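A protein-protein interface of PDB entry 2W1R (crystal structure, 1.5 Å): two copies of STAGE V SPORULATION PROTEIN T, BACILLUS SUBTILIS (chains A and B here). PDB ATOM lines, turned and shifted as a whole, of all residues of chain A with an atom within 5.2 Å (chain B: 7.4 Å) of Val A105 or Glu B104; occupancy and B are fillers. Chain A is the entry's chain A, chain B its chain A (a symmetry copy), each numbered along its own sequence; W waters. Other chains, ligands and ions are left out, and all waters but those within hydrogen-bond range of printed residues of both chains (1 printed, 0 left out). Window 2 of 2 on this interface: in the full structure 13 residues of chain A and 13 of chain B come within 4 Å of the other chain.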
ATOM      1  N   LEU A  15     -12.735  -0.377  30.566  1.00  0.00           N
ATOM      2  CA  LEU A  15     -12.045  -0.976  29.417  1.00  0.00           C
ATOM      3  C   LEU A  15     -12.854  -2.004  28.631  1.00  0.00           C
ATOM      4  O   LEU A  15     -12.564  -2.257  27.461  1.00  0.00           O
ATOM      5  CB  LEU A  15     -10.706  -1.576  29.848  1.00  0.00           C
ATOM      6  CG  LEU A  15      -9.793  -0.683  30.688  1.00  0.00           C
ATOM      7  CD1 LEU A  15      -8.540  -1.442  31.057  1.00  0.00           C
ATOM      8  CD2 LEU A  15      -9.447   0.610  29.961  1.00  0.00           C
ATOM      9  N   GLY A 103      -3.601  -3.838  24.332  1.00  0.00           N
ATOM     10  CA  GLY A 103      -2.528  -2.929  23.956  1.00  0.00           C
ATOM     11  C   GLY A 103      -1.982  -2.212  25.172  1.00  0.00           C
ATOM     12  O   GLY A 103      -2.165  -2.652  26.309  1.00  0.00           O
ATOM     13  N   GLU A 104      -1.307  -1.095  24.934  1.00  0.00           N
ATOM     14  CA  GLU A 104      -0.697  -0.342  26.029  1.00  0.00           C
ATOM     15  C   GLU A 104      -1.722   0.181  27.046  1.00  0.00           C
ATOM     16  O   GLU A 104      -1.421   0.297  28.234  1.00  0.00           O
ATOM     17  CB  GLU A 104       0.175   0.793  25.491  1.00  0.00           C
ATOM     18  CG  GLU A 104       1.091   1.410  26.542  1.00  0.00           C
ATOM     19  CD  GLU A 104       2.172   0.469  27.078  1.00  0.00           C
ATOM     20  OE1 GLU A 104       2.207  -0.732  26.722  1.00  0.00           O
ATOM     21  OE2 GLU A 104       3.015   0.952  27.864  1.00  0.00           O
ATOM     22  N   VAL A 105      -2.926   0.485  26.579  1.00  0.00           N
ATOM     23  CA  VAL A 105      -4.003   0.898  27.477  1.00  0.00           C
ATOM     24  C   VAL A 105      -4.185  -0.123  28.605  1.00  0.00           C
ATOM     25  O   VAL A 105      -4.150   0.230  29.784  1.00  0.00           O
ATOM     26  CB  VAL A 105      -5.330   1.072  26.712  1.00  0.00           C
ATOM     27  CG1 VAL A 105      -6.512   1.222  27.677  1.00  0.00           C
ATOM     28  CG2 VAL A 105      -5.239   2.270  25.769  1.00  0.00           C
ATOM     29  N   GLU A 106      -4.382  -1.384  28.230  1.00  0.00           N
ATOM     30  CA  GLU A 106      -4.611  -2.455  29.194  1.00  0.00           C
ATOM     31  C   GLU A 106      -3.334  -2.832  29.932  1.00  0.00           C
ATOM     32  O   GLU A 106      -3.367  -3.165  31.123  1.00  0.00           O
ATOM     33  CB  GLU A 106      -5.191  -3.681  28.491  1.00  0.00           C
ATOM     34  CG  GLU A 106      -6.585  -3.466  27.912  1.00  0.00           C
ATOM     35  CD  GLU A 106      -6.579  -2.763  26.561  1.00  0.00           C
ATOM     36  OE1 GLU A 106      -5.494  -2.589  25.957  1.00  0.00           O
ATOM     37  OE2 GLU A 106      -7.665  -2.386  26.098  1.00  0.00           O
ATOM     38  N   HIS A 107      -2.208  -2.790  29.216  1.00  0.00           N
ATOM     39  CA  HIS A 107      -0.906  -3.106  29.786  1.00  0.00           C
ATOM     40  C   HIS A 107      -0.586  -2.143  30.926  1.00  0.00           C
ATOM     41  O   HIS A 107      -0.204  -2.558  32.020  1.00  0.00           O
ATOM     42  CB  HIS A 107       0.145  -3.055  28.670  1.00  0.00           C
ATOM     43  CG  HIS A 107       1.552  -3.315  29.111  1.00  0.00           C
ATOM     44  ND1 HIS A 107       1.900  -4.300  30.009  1.00  0.00           N
ATOM     45  CD2 HIS A 107       2.710  -2.727  28.732  1.00  0.00           C
ATOM     46  CE1 HIS A 107       3.213  -4.302  30.169  1.00  0.00           C
ATOM     47  NE2 HIS A 107       3.727  -3.353  29.409  1.00  0.00           N
ATOM     48  N   LYS A 108      -0.774  -0.855  30.680  1.00  0.00           N
ATOM     49  CA  LYS A 108      -0.562   0.124  31.737  1.00  0.00           C
ATOM     50  C   LYS A 108      -1.632   0.049  32.813  1.00  0.00           C
ATOM     51  O   LYS A 108      -1.345   0.283  33.981  1.00  0.00           O
ATOM     52  CB  LYS A 108      -0.437   1.537  31.170  1.00  0.00           C
ATOM     53  CG  LYS A 108       0.845   1.749  30.352  1.00  0.00           C
ATOM     54  CD  LYS A 108       2.088   1.230  31.061  1.00  0.00           C
ATOM     55  CE  LYS A 108       2.538   2.148  32.159  1.00  0.00           C
ATOM     56  NZ  LYS A 108       3.964   1.875  32.530  1.00  0.00           N
ATOM     57  N   ALA A 109      -2.852  -0.305  32.420  1.00  0.00           N
ATOM     58  CA  ALA A 109      -3.941  -0.470  33.384  1.00  0.00           C
ATOM     59  C   ALA A 109      -3.596  -1.527  34.429  1.00  0.00           C
ATOM     60  O   ALA A 109      -3.819  -1.309  35.620  1.00  0.00           O
ATOM     61  CB  ALA A 109      -5.243  -0.814  32.689  1.00  0.00           C
ATOM     62  N   LEU B  15       2.506   5.685  35.074  1.00  0.00           N
ATOM     63  CA  LEU B  15       2.466   6.440  33.816  1.00  0.00           C
ATOM     64  C   LEU B  15       3.526   7.529  33.672  1.00  0.00           C
ATOM     65  O   LEU B  15       3.853   7.930  32.555  1.00  0.00           O
ATOM     66  CB  LEU B  15       1.072   7.027  33.586  1.00  0.00           C
ATOM     67  CG  LEU B  15      -0.110   6.070  33.741  1.00  0.00           C
ATOM     68  CD1 LEU B  15      -1.403   6.819  33.520  1.00  0.00           C
ATOM     69  CD2 LEU B  15      -0.002   4.885  32.789  1.00  0.00           C
ATOM     70  N   LEU B  58     -10.011  14.420  26.386  1.00  0.00           N
ATOM     71  CA  LEU B  58      -8.620  14.250  26.010  1.00  0.00           C
ATOM     72  C   LEU B  58      -8.226  15.379  25.074  1.00  0.00           C
ATOM     73  O   LEU B  58      -8.829  15.559  24.015  1.00  0.00           O
ATOM     74  CB  LEU B  58      -8.406  12.890  25.338  1.00  0.00           C
ATOM     75  CG  LEU B  58      -7.030  12.561  24.752  1.00  0.00           C
ATOM     76  CD1 LEU B  58      -5.928  12.559  25.812  1.00  0.00           C
ATOM     77  CD2 LEU B  58      -7.094  11.219  24.044  1.00  0.00           C
ATOM     78  N   THR B  79      -5.682  15.140  30.091  1.00  0.00           N
ATOM     79  CA  THR B  79      -6.895  14.358  30.024  1.00  0.00           C
ATOM     80  C   THR B  79      -7.606  14.430  31.375  1.00  0.00           C
ATOM     81  O   THR B  79      -6.953  14.528  32.424  1.00  0.00           O
ATOM     82  CB  THR B  79      -6.607  12.915  29.546  1.00  0.00           C
ATOM     83  OG1 THR B  79      -7.841  12.208  29.392  1.00  0.00           O
ATOM     84  CG2 THR B  79      -5.676  12.169  30.506  1.00  0.00           C
ATOM     85  N   THR B 101       2.713  13.768  25.117  1.00  0.00           N
ATOM     86  CA  THR B 101       1.359  13.725  24.596  1.00  0.00           C
ATOM     87  C   THR B 101       0.539  12.668  25.325  1.00  0.00           C
ATOM     88  O   THR B 101       0.910  11.499  25.357  1.00  0.00           O
ATOM     89  CB  THR B 101       1.349  13.437  23.077  1.00  0.00           C
ATOM     90  OG1 THR B 101       2.182  14.394  22.411  1.00  0.00           O
ATOM     91  CG2 THR B 101      -0.065  13.525  22.521  1.00  0.00           C
ATOM     92  N   MET B 102      -0.566  13.104  25.922  1.00  0.00           N
ATOM     93  CA  MET B 102      -1.519  12.194  26.536  1.00  0.00           C
ATOM     94  C   MET B 102      -2.252  11.479  25.420  1.00  0.00           C
ATOM     95  O   MET B 102      -2.654  12.095  24.432  1.00  0.00           O
ATOM     96  CB  MET B 102      -2.497  12.953  27.441  1.00  0.00           C
ATOM     97  CG  MET B 102      -1.820  13.789  28.531  1.00  0.00           C
ATOM     98  SD  MET B 102      -0.877  12.842  29.742  1.00  0.00           S
ATOM     99  CE  MET B 102       0.735  12.718  28.975  1.00  0.00           C
ATOM    100  N   GLY B 103      -2.380  10.168  25.572  1.00  0.00           N
ATOM    101  CA  GLY B 103      -3.090   9.346  24.602  1.00  0.00           C
ATOM    102  C   GLY B 103      -4.148   8.506  25.284  1.00  0.00           C
ATOM    103  O   GLY B 103      -4.574   8.800  26.402  1.00  0.00           O
ATOM    104  N   GLU B 104      -4.576   7.449  24.607  1.00  0.00           N
ATOM    105  CA  GLU B 104      -5.628   6.590  25.148  1.00  0.00           C
ATOM    106  C   GLU B 104      -5.235   5.915  26.470  1.00  0.00           C
ATOM    107  O   GLU B 104      -6.086   5.667  27.323  1.00  0.00           O
ATOM    108  CB  GLU B 104      -6.075   5.557  24.113  1.00  0.00           C
ATOM    109  CG  GLU B 104      -7.374   4.847  24.480  1.00  0.00           C
ATOM    110  CD  GLU B 104      -8.608   5.752  24.511  1.00  0.00           C
ATOM    111  OE1 GLU B 104      -8.499   6.987  24.334  1.00  0.00           O
ATOM    112  OE2 GLU B 104      -9.715   5.205  24.703  1.00  0.00           O
ATOM    113  N   VAL B 105      -3.949   5.631  26.637  1.00  0.00           N
ATOM    114  CA  VAL B 105      -3.455   5.077  27.896  1.00  0.00           C
ATOM    115  C   VAL B 105      -3.896   5.948  29.077  1.00  0.00           C
ATOM    116  O   VAL B 105      -4.506   5.457  30.028  1.00  0.00           O
ATOM    117  CB  VAL B 105      -1.918   4.953  27.885  1.00  0.00           C
ATOM    118  CG1 VAL B 105      -1.375   4.650  29.286  1.00  0.00           C
ATOM    119  CG2 VAL B 105      -1.485   3.881  26.887  1.00  0.00           C
ATOM    120  N   GLU B 106      -3.579   7.238  29.007  1.00  0.00           N
ATOM    121  CA  GLU B 106      -3.899   8.176  30.077  1.00  0.00           C
ATOM    122  C   GLU B 106      -5.386   8.504  30.115  1.00  0.00           C
ATOM    123  O   GLU B 106      -5.964   8.689  31.192  1.00  0.00           O
ATOM    124  CB  GLU B 106      -3.085   9.459  29.914  1.00  0.00           C
ATOM    125  CG  GLU B 106      -1.583   9.270  30.090  1.00  0.00           C
ATOM    126  CD  GLU B 106      -0.888   8.735  28.844  1.00  0.00           C
ATOM    127  OE1 GLU B 106      -1.517   8.672  27.762  1.00  0.00           O
ATOM    128  OE2 GLU B 106       0.296   8.383  28.947  1.00  0.00           O
ATOM    129  N   HIS B 107      -5.999   8.585  28.932  1.00  0.00           N
ATOM    130  CA  HIS B 107      -7.421   8.872  28.806  1.00  0.00           C
ATOM    131  C   HIS B 107      -8.238   7.789  29.506  1.00  0.00           C
ATOM    132  O   HIS B 107      -9.130   8.081  30.302  1.00  0.00           O
ATOM    133  CB  HIS B 107      -7.768   8.990  27.317  1.00  0.00           C
ATOM    134  CG  HIS B 107      -9.214   9.241  27.020  1.00  0.00           C
ATOM    135  ND1 HIS B 107      -9.998  10.121  27.734  1.00  0.00           N
ATOM    136  CD2 HIS B 107     -10.007   8.740  26.044  1.00  0.00           C
ATOM    137  CE1 HIS B 107     -11.213  10.146  27.214  1.00  0.00           C
ATOM    138  NE2 HIS B 107     -11.245   9.314  26.190  1.00  0.00           N
ATOM    139  N   LYS B 108      -7.909   6.535  29.234  1.00  0.00           N
ATOM    140  CA  LYS B 108      -8.591   5.443  29.915  1.00  0.00           C
ATOM    141  C   LYS B 108      -8.207   5.353  31.383  1.00  0.00           C
ATOM    142  O   LYS B 108      -9.033   4.989  32.211  1.00  0.00           O
ATOM    143  CB  LYS B 108      -8.369   4.113  29.196  1.00  0.00           C
ATOM    144  CG  LYS B 108      -9.060   4.044  27.827  1.00  0.00           C
ATOM    145  CD  LYS B 108     -10.507   4.514  27.874  1.00  0.00           C
ATOM    146  CE  LYS B 108     -11.417   3.485  28.478  1.00  0.00           C
ATOM    147  NZ  LYS B 108     -12.845   3.757  28.115  1.00  0.00           N
ATOM    148  N   ALA B 109      -6.967   5.712  31.700  1.00  0.00           N
ATOM    149  CA  ALA B 109      -6.514   5.723  33.092  1.00  0.00           C
ATOM    150  C   ALA B 109      -7.371   6.658  33.941  1.00  0.00           C
ATOM    151  O   ALA B 109      -7.768   6.291  35.048  1.00  0.00           O
ATOM    152  CB  ALA B 109      -5.051   6.107  33.191  1.00  0.00           C
ATOM    153  N   VAL B 110      -7.675   7.848  33.429  1.00  0.00           N
ATOM    154  CA  VAL B 110      -8.500   8.768  34.222  1.00  0.00           C
ATOM    155  C   VAL B 110      -9.933   8.274  34.359  1.00  0.00           C
ATOM    156  O   VAL B 110     -10.553   8.479  35.401  1.00  0.00           O
ATOM    157  CB  VAL B 110      -8.453  10.255  33.751  1.00  0.00           C
ATOM    158  CG1 VAL B 110      -7.052  10.836  33.908  1.00  0.00           C
ATOM    159  CG2 VAL B 110      -8.956  10.415  32.320  1.00  0.00           C
ATOM    160  N   GLU B 111     -10.453   7.616  33.317  1.00  0.00           N
ATOM    161  CA  GLU B 111     -11.795   7.052  33.387  1.00  0.00           C
ATOM    162  C   GLU B 111     -11.833   5.910  34.397  1.00  0.00           C
ATOM    163  O   GLU B 111     -12.739   5.841  35.223  1.00  0.00           O
ATOM    164  CB  GLU B 111     -12.276   6.578  32.016  1.00  0.00           C
ATOM    165  CG  GLU B 111     -13.717   6.086  32.034  1.00  0.00           C
ATOM    166  CD  GLU B 111     -14.164   5.478  30.724  1.00  0.00           C
ATOM    167  OE1 GLU B 111     -13.573   5.803  29.673  1.00  0.00           O
ATOM    168  OE2 GLU B 111     -15.123   4.675  30.747  1.00  0.00           O
ATOM    169  N   THR B 112     -10.834   5.036  34.340  1.00  0.00           N
ATOM    170  CA  THR B 112     -10.743   3.931  35.284  1.00  0.00           C
ATOM    171  C   THR B 112     -10.625   4.443  36.715  1.00  0.00           C
ATOM    172  O   THR B 112     -11.337   3.973  37.611  1.00  0.00           O
ATOM    173  CB  THR B 112      -9.549   3.026  34.955  1.00  0.00           C
ATOM    174  OG1 THR B 112      -9.734   2.469  33.652  1.00  0.00           O
ATOM    175  CG2 THR B 112      -9.451   1.899  35.966  1.00  0.00           C
HETATM  176  O   HOH W   1      -4.633   2.768  31.034  1.00  0.00           O
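OG1 of Thr B112 sits at hydrogen-bond distance from O of Lys B108, at 3.0 Å. NZ of Lys B108 lies within salt-bridge range of OE1 of Glu B111, at 2.7 Å.
Water W1 bridges O of Val A105 (2.9 Å) and O of Val B105 (2.9 Å).
Among the printed residues, merely in contact across the chains: Glu A104 with Val B105 (3.6 Å), Val A105 with Glu B104 (3.6 Å), Val A105 with Val B105 (3.7 Å), Leu A15 with Lys B108 (3.7 Å), Lys A108 with Leu B15 (3.7 Å), Val A105 with Lys B108 (3.8 Å) and Lys A108 with Val B105 (3.8 Å).
Hydrophobic or aromatic side chains of chain A that line the printed part of chain B: Leu A15 and Val A105. Of the 15 printed residues of chain B, 4 touch a printed residue of chain A. Hydrophobic or aromatic side chains of chain B within 4 Å of the printed part of chain A: Leu B15 and Val B105. Among the printed residues, no Asp or Glu carboxylate lies within 4 Å of a Lys or Arg side-chain nitrogen of the other chain.
Printed residues of chain B within 4 Å of Leu A15: Lys B108 (3.7 Å). Of the printed residues of chain B, Glu A104 touches Val B105. His A107 touches none of the printed residues of chain B. Printed residues of chain A within 4 Å of Leu B15: Lys A108 (3.7 Å). Of the printed residues of chain A, Val B105 touches Glu A104, Val A105 and Lys A108. Of the printed residues of chain A, Lys B108 touches Leu A15 (3.7 Å) and Val A105 (3.8 Å). The nearest residue of chain B that does not touch Val A105 is Ala B109 (6.0 Å). The nearest printed residue of chain A that does not touch Glu B104 is Leu A15 (6.6 Å). The nearest printed residue of chain A that does not touch Lys B108 is Ala A109 (6.8 Å).
Leu A15 touches Lys B108, and with the chains exchanged Lys A108 touches Leu B15. Glu A104 touches Val B105, and with the chains exchanged Val A105 touches Glu B104. Val B105 touches its own counterpart, Val A105. Val A105 touches Lys B108, and with the chains exchanged Lys A108 touches Val B105. Positions printed for both chains: 15, 103, 104, 105, 106, 107, 108 and 109. Of the 7 pairs that touch across the chains among the printed residues, 7 have their exchanged pair printed and touching as well.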
